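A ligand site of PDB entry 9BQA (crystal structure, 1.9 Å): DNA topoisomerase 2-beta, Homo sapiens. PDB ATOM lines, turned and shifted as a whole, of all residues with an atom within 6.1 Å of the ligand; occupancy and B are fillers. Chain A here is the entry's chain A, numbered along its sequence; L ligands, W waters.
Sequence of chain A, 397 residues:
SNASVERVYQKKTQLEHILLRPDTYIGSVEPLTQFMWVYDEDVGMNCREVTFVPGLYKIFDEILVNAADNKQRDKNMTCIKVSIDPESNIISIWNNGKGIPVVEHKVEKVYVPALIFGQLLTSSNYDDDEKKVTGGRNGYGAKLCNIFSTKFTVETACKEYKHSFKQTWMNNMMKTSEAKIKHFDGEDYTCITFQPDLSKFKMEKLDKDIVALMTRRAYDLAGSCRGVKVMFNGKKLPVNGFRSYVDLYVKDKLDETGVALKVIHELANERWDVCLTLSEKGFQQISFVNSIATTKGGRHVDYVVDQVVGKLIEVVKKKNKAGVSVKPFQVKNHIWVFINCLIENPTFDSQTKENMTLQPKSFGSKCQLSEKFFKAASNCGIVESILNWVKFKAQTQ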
ATOM      1  N   LEU A  32      11.427 -14.780  19.397  1.00  0.00           N
ATOM      2  CA  LEU A  32      11.973 -13.780  18.501  1.00  0.00           C
ATOM      3  C   LEU A  32      11.257 -12.452  18.706  1.00  0.00           C
ATOM      4  O   LEU A  32      10.020 -12.418  18.786  1.00  0.00           O
ATOM      5  CB  LEU A  32      11.800 -14.217  17.040  1.00  0.00           C
ATOM      6  CG  LEU A  32      12.169 -13.216  15.954  1.00  0.00           C
ATOM      7  CD1 LEU A  32      13.644 -12.885  16.017  1.00  0.00           C
ATOM      8  CD2 LEU A  32      11.793 -13.778  14.586  1.00  0.00           C
ATOM      9  N   GLN A  34      10.785  -8.685  16.932  1.00  0.00           N
ATOM     10  CA  GLN A  34      11.056  -7.876  15.754  1.00  0.00           C
ATOM     11  C   GLN A  34       9.848  -7.022  15.411  1.00  0.00           C
ATOM     12  O   GLN A  34       8.714  -7.315  15.811  1.00  0.00           O
ATOM     13  CB  GLN A  34      11.429  -8.748  14.563  1.00  0.00           C
ATOM     14  CG  GLN A  34      10.261  -9.548  14.067  1.00  0.00           C
ATOM     15  CD  GLN A  34      10.637 -10.482  12.959  1.00  0.00           C
ATOM     16  OE1 GLN A  34      11.825 -10.695  12.670  1.00  0.00           O
ATOM     17  NE2 GLN A  34       9.636 -11.060  12.316  1.00  0.00           N
ATOM     18  N   PHE A  35      10.105  -5.972  14.635  1.00  0.00           N
ATOM     19  CA  PHE A  35       9.051  -5.120  14.116  1.00  0.00           C
ATOM     20  C   PHE A  35       8.365  -5.825  12.958  1.00  0.00           C
ATOM     21  O   PHE A  35       9.019  -6.388  12.083  1.00  0.00           O
ATOM     22  CB  PHE A  35       9.618  -3.780  13.644  1.00  0.00           C
ATOM     23  CG  PHE A  35       9.649  -2.730  14.722  1.00  0.00           C
ATOM     24  CD1 PHE A  35       8.543  -1.932  14.954  1.00  0.00           C
ATOM     25  CD2 PHE A  35      10.786  -2.553  15.486  1.00  0.00           C
ATOM     26  CE1 PHE A  35       8.568  -0.965  15.941  1.00  0.00           C
ATOM     27  CE2 PHE A  35      10.818  -1.579  16.482  1.00  0.00           C
ATOM     28  CZ  PHE A  35       9.706  -0.788  16.705  1.00  0.00           C
ATOM     29  N   MET A  36       7.036  -5.795  12.959  1.00  0.00           N
ATOM     30  CA  MET A  36       6.273  -6.441  11.889  1.00  0.00           C
ATOM     31  C   MET A  36       4.817  -6.034  12.043  1.00  0.00           C
ATOM     32  O   MET A  36       4.450  -5.291  12.967  1.00  0.00           O
ATOM     33  CB  MET A  36       6.428  -7.951  11.922  1.00  0.00           C
ATOM     34  CG  MET A  36       6.023  -8.555  13.258  1.00  0.00           C
ATOM     35  SD  MET A  36       6.270 -10.332  13.331  1.00  0.00           S
ATOM     36  CE  MET A  36       5.116 -10.881  12.066  1.00  0.00           C
ATOM     37  N   TRP A  37       3.994  -6.540  11.156  1.00  0.00           N
ATOM     38  CA  TRP A  37       2.580  -6.216  11.104  1.00  0.00           C
ATOM     39  C   TRP A  37       1.807  -7.330  11.809  1.00  0.00           C
ATOM     40  O   TRP A  37       2.046  -8.513  11.569  1.00  0.00           O
ATOM     41  CB  TRP A  37       2.110  -6.061   9.656  1.00  0.00           C
ATOM     42  CG  TRP A  37       2.838  -4.967   8.914  1.00  0.00           C
ATOM     43  CD1 TRP A  37       3.984  -5.096   8.160  1.00  0.00           C
ATOM     44  CD2 TRP A  37       2.470  -3.588   8.850  1.00  0.00           C
ATOM     45  NE1 TRP A  37       4.330  -3.875   7.633  1.00  0.00           N
ATOM     46  CE2 TRP A  37       3.430  -2.934   8.038  1.00  0.00           C
ATOM     47  CE3 TRP A  37       1.416  -2.837   9.389  1.00  0.00           C
ATOM     48  CZ2 TRP A  37       3.353  -1.567   7.765  1.00  0.00           C
ATOM     49  CZ3 TRP A  37       1.360  -1.481   9.112  1.00  0.00           C
ATOM     50  CH2 TRP A  37       2.322  -0.862   8.306  1.00  0.00           C
ATOM     51  N   VAL A  38       0.917  -6.938  12.706  1.00  0.00           N
ATOM     52  CA  VAL A  38      -0.007  -7.867  13.331  1.00  0.00           C
ATOM     53  C   VAL A  38      -1.369  -7.181  13.407  1.00  0.00           C
ATOM     54  O   VAL A  38      -1.488  -5.977  13.172  1.00  0.00           O
ATOM     55  CB  VAL A  38       0.459  -8.323  14.733  1.00  0.00           C
ATOM     56  CG1 VAL A  38       1.732  -9.152  14.621  1.00  0.00           C
ATOM     57  CG2 VAL A  38       0.678  -7.123  15.628  1.00  0.00           C
ATOM     58  N   PHE A  52       7.383 -13.395  19.597  1.00  0.00           N
ATOM     59  CA  PHE A  52       6.684 -14.640  19.316  1.00  0.00           C
ATOM     60  C   PHE A  52       7.688 -15.723  18.994  1.00  0.00           C
ATOM     61  O   PHE A  52       8.859 -15.457  18.709  1.00  0.00           O
ATOM     62  CB  PHE A  52       5.710 -14.451  18.165  1.00  0.00           C
ATOM     63  CG  PHE A  52       6.380 -14.290  16.838  1.00  0.00           C
ATOM     64  CD1 PHE A  52       7.016 -13.100  16.507  1.00  0.00           C
ATOM     65  CD2 PHE A  52       6.378 -15.325  15.908  1.00  0.00           C
ATOM     66  CE1 PHE A  52       7.630 -12.955  15.264  1.00  0.00           C
ATOM     67  CE2 PHE A  52       6.982 -15.184  14.674  1.00  0.00           C
ATOM     68  CZ  PHE A  52       7.608 -14.000  14.352  1.00  0.00           C
ATOM     69  N   PRO A  54       8.637 -18.471  16.327  1.00  0.00           N
ATOM     70  CA  PRO A  54       8.306 -18.776  14.928  1.00  0.00           C
ATOM     71  C   PRO A  54       7.675 -20.147  14.701  1.00  0.00           C
ATOM     72  O   PRO A  54       6.735 -20.264  13.894  1.00  0.00           O
ATOM     73  CB  PRO A  54       9.661 -18.657  14.217  1.00  0.00           C
ATOM     74  CG  PRO A  54      10.422 -17.643  15.063  1.00  0.00           C
ATOM     75  CD  PRO A  54      10.009 -17.967  16.487  1.00  0.00           C
ATOM     76  N   TYR A  57       3.871 -20.045  15.337  1.00  0.00           N
ATOM     77  CA  TYR A  57       3.268 -19.433  14.151  1.00  0.00           C
ATOM     78  C   TYR A  57       3.187 -20.427  13.003  1.00  0.00           C
ATOM     79  O   TYR A  57       2.152 -20.568  12.357  1.00  0.00           O
ATOM     80  CB  TYR A  57       4.067 -18.172  13.778  1.00  0.00           C
ATOM     81  CG  TYR A  57       4.060 -17.777  12.311  1.00  0.00           C
ATOM     82  CD1 TYR A  57       2.893 -17.372  11.666  1.00  0.00           C
ATOM     83  CD2 TYR A  57       5.236 -17.766  11.562  1.00  0.00           C
ATOM     84  CE1 TYR A  57       2.894 -16.984  10.326  1.00  0.00           C
ATOM     85  CE2 TYR A  57       5.250 -17.395  10.216  1.00  0.00           C
ATOM     86  CZ  TYR A  57       4.076 -16.999   9.602  1.00  0.00           C
ATOM     87  OH  TYR A  57       4.086 -16.625   8.276  1.00  0.00           O
ATOM     88  N   LEU A 213      -0.623 -12.171  15.563  1.00  0.00           N
ATOM     89  CA  LEU A 213       0.012 -12.660  14.342  1.00  0.00           C
ATOM     90  C   LEU A 213      -0.836 -13.706  13.650  1.00  0.00           C
ATOM     91  O   LEU A 213      -1.062 -13.642  12.440  1.00  0.00           O
ATOM     92  CB  LEU A 213       1.393 -13.214  14.693  1.00  0.00           C
ATOM     93  CG  LEU A 213       2.173 -13.918  13.596  1.00  0.00           C
ATOM     94  CD1 LEU A 213       2.277 -13.112  12.313  1.00  0.00           C
ATOM     95  CD2 LEU A 213       3.569 -14.249  14.131  1.00  0.00           C
ATOM     96  N   ARG A 216      -3.687 -11.905  12.027  1.00  0.00           N
ATOM     97  CA  ARG A 216      -3.330 -11.232  10.784  1.00  0.00           C
ATOM     98  C   ARG A 216      -3.235 -12.224   9.630  1.00  0.00           C
ATOM     99  O   ARG A 216      -3.616 -11.903   8.503  1.00  0.00           O
ATOM    100  CB  ARG A 216      -2.011 -10.478  10.925  1.00  0.00           C
ATOM    101  CG  ARG A 216      -1.857  -9.368   9.882  1.00  0.00           C
ATOM    102  CD  ARG A 216      -0.417  -9.232   9.392  1.00  0.00           C
ATOM    103  NE  ARG A 216      -0.009 -10.442   8.694  1.00  0.00           N
ATOM    104  CZ  ARG A 216       1.017 -11.194   9.058  1.00  0.00           C
ATOM    105  NH1 ARG A 216       1.839 -10.843  10.031  1.00  0.00           N
ATOM    106  NH2 ARG A 216       1.213 -12.350   8.423  1.00  0.00           N
ATOM    107  N   ARG A 217      -2.728 -13.441   9.881  1.00  0.00           N
ATOM    108  CA  ARG A 217      -2.676 -14.417   8.798  1.00  0.00           C
ATOM    109  C   ARG A 217      -4.072 -14.707   8.259  1.00  0.00           C
ATOM    110  O   ARG A 217      -4.239 -14.966   7.071  1.00  0.00           O
ATOM    111  CB  ARG A 217      -2.013 -15.723   9.260  1.00  0.00           C
ATOM    112  CG  ARG A 217      -0.489 -15.654   9.354  1.00  0.00           C
ATOM    113  CD  ARG A 217       0.231 -15.519   7.989  1.00  0.00           C
ATOM    114  NE  ARG A 217       0.073 -16.687   7.132  1.00  0.00           N
ATOM    115  CZ  ARG A 217      -0.424 -16.680   5.899  1.00  0.00           C
ATOM    116  NH1 ARG A 217      -0.771 -15.555   5.291  1.00  0.00           N
ATOM    117  NH2 ARG A 217      -0.550 -17.828   5.241  1.00  0.00           N
ATOM    118  N   ASP A 220      -4.611 -11.967   5.996  1.00  0.00           N
ATOM    119  CA  ASP A 220      -3.809 -12.232   4.803  1.00  0.00           C
ATOM    120  C   ASP A 220      -4.585 -13.115   3.831  1.00  0.00           C
ATOM    121  O   ASP A 220      -4.630 -12.877   2.619  1.00  0.00           O
ATOM    122  CB  ASP A 220      -2.514 -12.969   5.145  1.00  0.00           C
ATOM    123  CG  ASP A 220      -1.535 -12.151   5.951  1.00  0.00           C
ATOM    124  OD1 ASP A 220      -1.744 -10.945   6.234  1.00  0.00           O
ATOM    125  OD2 ASP A 220      -0.520 -12.774   6.302  1.00  0.00           O
ATOM    126  N   TYR A 245      -7.341  -5.526   1.052  1.00  0.00           N
ATOM    127  CA  TYR A 245      -6.350  -5.964   2.018  1.00  0.00           C
ATOM    128  C   TYR A 245      -5.198  -4.972   2.088  1.00  0.00           C
ATOM    129  O   TYR A 245      -4.783  -4.547   3.165  1.00  0.00           O
ATOM    130  CB  TYR A 245      -5.850  -7.356   1.636  1.00  0.00           C
ATOM    131  CG  TYR A 245      -4.663  -7.804   2.468  1.00  0.00           C
ATOM    132  CD1 TYR A 245      -4.833  -8.390   3.703  1.00  0.00           C
ATOM    133  CD2 TYR A 245      -3.370  -7.629   2.004  1.00  0.00           C
ATOM    134  CE1 TYR A 245      -3.761  -8.781   4.462  1.00  0.00           C
ATOM    135  CE2 TYR A 245      -2.289  -8.016   2.753  1.00  0.00           C
ATOM    136  CZ  TYR A 245      -2.485  -8.598   3.983  1.00  0.00           C
ATOM    137  OH  TYR A 245      -1.406  -8.998   4.734  1.00  0.00           O
ATOM    138  N   TYR A 249      -3.029  -1.440   5.113  1.00  0.00           N
ATOM    139  CA  TYR A 249      -1.691  -0.915   5.346  1.00  0.00           C
ATOM    140  C   TYR A 249      -1.530   0.547   4.970  1.00  0.00           C
ATOM    141  O   TYR A 249      -0.821   1.282   5.664  1.00  0.00           O
ATOM    142  CB  TYR A 249      -0.648  -1.726   4.556  1.00  0.00           C
ATOM    143  CG  TYR A 249      -0.529  -3.147   5.011  1.00  0.00           C
ATOM    144  CD1 TYR A 249      -1.373  -4.138   4.527  1.00  0.00           C
ATOM    145  CD2 TYR A 249       0.443  -3.524   5.933  1.00  0.00           C
ATOM    146  CE1 TYR A 249      -1.264  -5.446   4.952  1.00  0.00           C
ATOM    147  CE2 TYR A 249       0.558  -4.824   6.368  1.00  0.00           C
ATOM    148  CZ  TYR A 249      -0.297  -5.784   5.887  1.00  0.00           C
ATOM    149  OH  TYR A 249      -0.159  -7.082   6.317  1.00  0.00           O
ATOM    150  N   GLN A 285       8.552  -5.046   1.276  1.00  0.00           N
ATOM    151  CA  GLN A 285       7.722  -5.889   0.442  1.00  0.00           C
ATOM    152  C   GLN A 285       6.761  -6.679   1.316  1.00  0.00           C
ATOM    153  O   GLN A 285       7.137  -7.151   2.383  1.00  0.00           O
ATOM    154  CB  GLN A 285       8.548  -6.856  -0.408  1.00  0.00           C
ATOM    155  CG  GLN A 285       9.315  -7.903   0.384  1.00  0.00           C
ATOM    156  CD  GLN A 285       8.524  -9.180   0.647  1.00  0.00           C
ATOM    157  OE1 GLN A 285       7.403  -9.357   0.176  1.00  0.00           O
ATOM    158  NE2 GLN A 285       9.119 -10.084   1.403  1.00  0.00           N
ATOM    159  N   ILE A 286       5.515  -6.794   0.851  1.00  0.00           N
ATOM    160  CA  ILE A 286       4.535  -7.724   1.403  1.00  0.00           C
ATOM    161  C   ILE A 286       4.078  -8.593   0.244  1.00  0.00           C
ATOM    162  O   ILE A 286       3.512  -8.081  -0.733  1.00  0.00           O
ATOM    163  CB  ILE A 286       3.369  -6.990   2.078  1.00  0.00           C
ATOM    164  CG1 ILE A 286       3.873  -6.375   3.390  1.00  0.00           C
ATOM    165  CG2 ILE A 286       2.213  -7.941   2.320  1.00  0.00           C
ATOM    166  CD1 ILE A 286       3.013  -5.270   3.932  1.00  0.00           C
ATOM    167  N   SER A 287       4.333  -9.894   0.335  1.00  0.00           N
ATOM    168  CA  SER A 287       4.076 -10.760  -0.806  1.00  0.00           C
ATOM    169  C   SER A 287       3.544 -12.109  -0.367  1.00  0.00           C
ATOM    170  O   SER A 287       3.831 -12.601   0.728  1.00  0.00           O
ATOM    171  CB  SER A 287       5.358 -10.977  -1.632  1.00  0.00           C
ATOM    172  OG  SER A 287       6.367 -11.585  -0.841  1.00  0.00           O
ATOM    173  N   PHE A 288       2.746 -12.712  -1.254  1.00  0.00           N
ATOM    174  CA  PHE A 288       2.146 -14.017  -1.052  1.00  0.00           C
ATOM    175  C   PHE A 288       2.317 -14.834  -2.322  1.00  0.00           C
ATOM    176  O   PHE A 288       2.131 -14.325  -3.440  1.00  0.00           O
ATOM    177  CB  PHE A 288       0.660 -13.902  -0.682  1.00  0.00           C
ATOM    178  CG  PHE A 288       0.415 -13.014   0.500  1.00  0.00           C
ATOM    179  CD1 PHE A 288       0.433 -13.535   1.783  1.00  0.00           C
ATOM    180  CD2 PHE A 288       0.221 -11.653   0.329  1.00  0.00           C
ATOM    181  CE1 PHE A 288       0.236 -12.716   2.873  1.00  0.00           C
ATOM    182  CE2 PHE A 288       0.032 -10.828   1.419  1.00  0.00           C
ATOM    183  CZ  PHE A 288       0.044 -11.357   2.692  1.00  0.00           C
ATOM    184  N   ALA A 293       2.676 -16.531   3.062  1.00  0.00           N
ATOM    185  CA  ALA A 293       3.360 -15.258   3.263  1.00  0.00           C
ATOM    186  C   ALA A 293       4.858 -15.451   3.033  1.00  0.00           C
ATOM    187  O   ALA A 293       5.545 -16.088   3.847  1.00  0.00           O
ATOM    188  CB  ALA A 293       3.098 -14.713   4.673  1.00  0.00           C
ATOM    189  N   THR A 294       5.378 -14.921   1.927  1.00  0.00           N
ATOM    190  CA  THR A 294       6.806 -15.079   1.605  1.00  0.00           C
ATOM    191  C   THR A 294       7.596 -13.956   2.274  1.00  0.00           C
ATOM    192  O   THR A 294       7.977 -12.951   1.674  1.00  0.00           O
ATOM    193  CB  THR A 294       7.023 -15.133   0.098  1.00  0.00           C
ATOM    194  OG1 THR A 294       6.258 -14.103  -0.546  1.00  0.00           O
ATOM    195  CG2 THR A 294       6.581 -16.487  -0.455  1.00  0.00           C
ATOM    196  N   THR A 295       7.867 -14.167   3.567  1.00  0.00           N
ATOM    197  CA  THR A 295       8.363 -13.091   4.423  1.00  0.00           C
ATOM    198  C   THR A 295       9.839 -12.801   4.225  1.00  0.00           C
ATOM    199  O   THR A 295      10.324 -11.794   4.759  1.00  0.00           O
ATOM    200  CB  THR A 295       8.063 -13.448   5.885  1.00  0.00           C
ATOM    201  OG1 THR A 295       8.418 -14.814   6.151  1.00  0.00           O
ATOM    202  CG2 THR A 295       6.566 -13.279   6.161  1.00  0.00           C
ATOM    203  N   LYS A 296      10.559 -13.605   3.453  1.00  0.00           N
ATOM    204  CA  LYS A 296      11.891 -13.249   2.978  1.00  0.00           C
ATOM    205  C   LYS A 296      11.897 -12.887   1.499  1.00  0.00           C
ATOM    206  O   LYS A 296      12.973 -12.620   0.947  1.00  0.00           O
ATOM    207  CB  LYS A 296      12.861 -14.410   3.241  1.00  0.00           C
ATOM    208  CG  LYS A 296      13.284 -14.522   4.693  1.00  0.00           C
ATOM    209  CD  LYS A 296      14.240 -15.693   4.913  1.00  0.00           C
ATOM    210  CE  LYS A 296      14.338 -16.058   6.383  1.00  0.00           C
ATOM    211  NZ  LYS A 296      14.784 -14.899   7.215  1.00  0.00           N
ATOM    212  N   GLY A 297      10.743 -12.890   0.838  1.00  0.00           N
ATOM    213  CA  GLY A 297      10.644 -12.545  -0.567  1.00  0.00           C
ATOM    214  C   GLY A 297      10.913 -13.720  -1.483  1.00  0.00           C
ATOM    215  O   GLY A 297      10.511 -14.847  -1.187  1.00  0.00           O
ATOM    216  N   GLU A 354       9.610 -19.182   3.490  1.00  0.00           N
ATOM    217  CA  GLU A 354       9.757 -17.729   3.577  1.00  0.00           C
ATOM    218  C   GLU A 354      10.342 -17.136   2.309  1.00  0.00           C
ATOM    219  O   GLU A 354      10.095 -15.957   2.011  1.00  0.00           O
ATOM    220  CB  GLU A 354      10.638 -17.345   4.763  1.00  0.00           C
ATOM    221  CG  GLU A 354      10.104 -17.702   6.127  1.00  0.00           C
ATOM    222  CD  GLU A 354      10.778 -16.914   7.250  1.00  0.00           C
ATOM    223  OE1 GLU A 354      10.794 -15.654   7.197  1.00  0.00           O
ATOM    224  OE2 GLU A 354      11.302 -17.547   8.186  1.00  0.00           O
HETATM  225  C1  LIG L   1       9.413 -15.951  11.129  1.00  0.00           C
HETATM  226  C2  LIG L   1       6.224 -10.987   8.836  1.00  0.00           C
HETATM  227  C3  LIG L   1       1.956  -9.602   5.896  1.00  0.00           C
HETATM  228  C4  LIG L   1       8.564 -10.876   9.125  1.00  0.00           C
HETATM  229  O1  LIG L   1       9.713 -11.506   9.462  1.00  0.00           O
HETATM  230  C5  LIG L   1       6.160  -9.656   8.416  1.00  0.00           C
HETATM  231  O2  LIG L   1       7.185  -7.651   7.980  1.00  0.00           O
HETATM  232  C6  LIG L   1       8.547  -9.542   8.724  1.00  0.00           C
HETATM  233  C7  LIG L   1       7.340  -8.933   8.379  1.00  0.00           C
HETATM  234  C8  LIG L   1       8.152 -15.257  10.605  1.00  0.00           C
HETATM  235  C9  LIG L   1       8.470 -13.877   9.995  1.00  0.00           C
HETATM  236  C10 LIG L   1      10.944 -10.915   9.075  1.00  0.00           C
HETATM  237  C11 LIG L   1       7.277 -13.054   9.598  1.00  0.00           C
HETATM  238  C12 LIG L   1       4.859 -12.925   9.234  1.00  0.00           C
HETATM  239  C13 LIG L   1       4.764  -9.787   5.706  1.00  0.00           C
HETATM  240  C14 LIG L   1       6.050 -13.629   9.602  1.00  0.00           C
HETATM  241  C15 LIG L   1       7.383 -11.665   9.203  1.00  0.00           C
HETATM  242  C16 LIG L   1       4.430 -11.201   3.811  1.00  0.00           C
HETATM  243  C17 LIG L   1       3.966 -10.668   5.007  1.00  0.00           C
HETATM  244  C18 LIG L   1       2.861  -8.676   6.732  1.00  0.00           C
HETATM  245  C19 LIG L   1       2.609 -10.951   5.568  1.00  0.00           C
HETATM  246  C20 LIG L   1       6.497  -9.966   4.065  1.00  0.00           C
HETATM  247  C21 LIG L   1       5.700 -10.864   3.348  1.00  0.00           C
HETATM  248  C22 LIG L   1       8.276  -6.737   8.154  1.00  0.00           C
HETATM  249  C23 LIG L   1       6.034  -9.419   5.259  1.00  0.00           C
HETATM  250  C24 LIG L   1       4.808  -9.093   8.111  1.00  0.00           C
HETATM  251  N1  LIG L   1       4.210  -9.235   6.891  1.00  0.00           N
HETATM  252  O3  LIG L   1       3.730 -13.381   9.218  1.00  0.00           O
HETATM  253  O4  LIG L   1       4.214  -8.563   9.024  1.00  0.00           O
HETATM  254  O5  LIG L   1       5.003 -11.605   8.857  1.00  0.00           O
HETATM  255  O   HOH W   1       8.720 -18.471   8.906  1.00  0.00           O
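Met 36 touches the ligand (CE to O5, 3.3 Å).
CZ of Phe 52 touches C8 of the ligand (3.99 Å).
Leu 213 touches the ligand.
Asp 220 touches the ligand (OD2 to C19, 3.7 Å).
Tyr 245 touches the ligand (OH to C3, 3.6 Å).
OH of Tyr 249 touches C3 of the ligand (3.3 Å).
Gln 285 touches the ligand.
Ile 286 touches the ligand.
O of Ser 287 touches C16 of the ligand (3.4 Å).
Phe 288 touches the ligand (CZ to C19, 3.9 Å).
CB of Ala 293 touches C16 of the ligand (3.9 Å).
Thr 294 touches the ligand (O to C21, 3.5 Å).
CG2 of Thr 295 touches C14 of the ligand, 3.5 Å away.
OE2 of Glu 354 touches C1 of the ligand, 3.8 Å away.
Hydrophobic or aromatic side chains within 4 Å of the ligand: Met 36, Trp 37, Phe 52, Tyr 57, Leu 213, Ile 286, Phe 288 and Ala 293.
Within 4 Å of the ligand: Gln 34, Met 36, Trp 37, Phe 52, Tyr 57, Leu 213, Arg 216, Asp 220, Tyr 245, Tyr 249, Gln 285, Ile 286, Ser 287, Phe 288, Ala 293, Thr 294, Thr 295 and Glu 354.
The nearest printed residue that does not touch the ligand is Phe 35 (4.01 Å).
O3 of the ligand sits at hydrogen-bond distance from OH of Tyr 57, 3.4 Å away.
The guanidinium group (NH2) of Arg 216 is in hydrogen-bond range of an oxygen (O3) of the ligand (2.8 Å).
An oxygen (O4) of the ligand is in hydrogen-bond range of the backbone NH (N) of Trp 37, 2.9 Å away.
NE2 of Gln 34 sits at hydrogen-bond distance from O1 of the ligand (2.9 Å).
OG of Ser 287 is in hydrogen-bond range of OE1 of Gln 285, 2.7 Å away.
SD of Met 36 sits at hydrogen-bond distance from NE2 of Gln 34 (3.6 Å).
The side-chain amide nitrogen of Gln 285 sits at hydrogen-bond distance from the backbone carbonyl oxygen of Thr 294 (3.1 Å).
The side-chain carboxylate (OD2) of Asp 220 is in salt-bridge range of the guanidinium group (NH1) of Arg 217 (3.0 Å).
The side-chain hydroxyl of Tyr 249 is in hydrogen-bond range of the side-chain hydroxyl of Tyr 245 (2.8 Å).
N of Leu 32 sits at hydrogen-bond distance from O of Phe 52 (2.7 Å).
The guanidinium group (NH2) of Arg 216 is in salt-bridge range of the side-chain carboxylate (OD2) of Asp 220 (2.8 Å).
OG1 of Thr 295 lies within hydrogen-bond range of OE1 of Glu 354 (2.7 Å).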
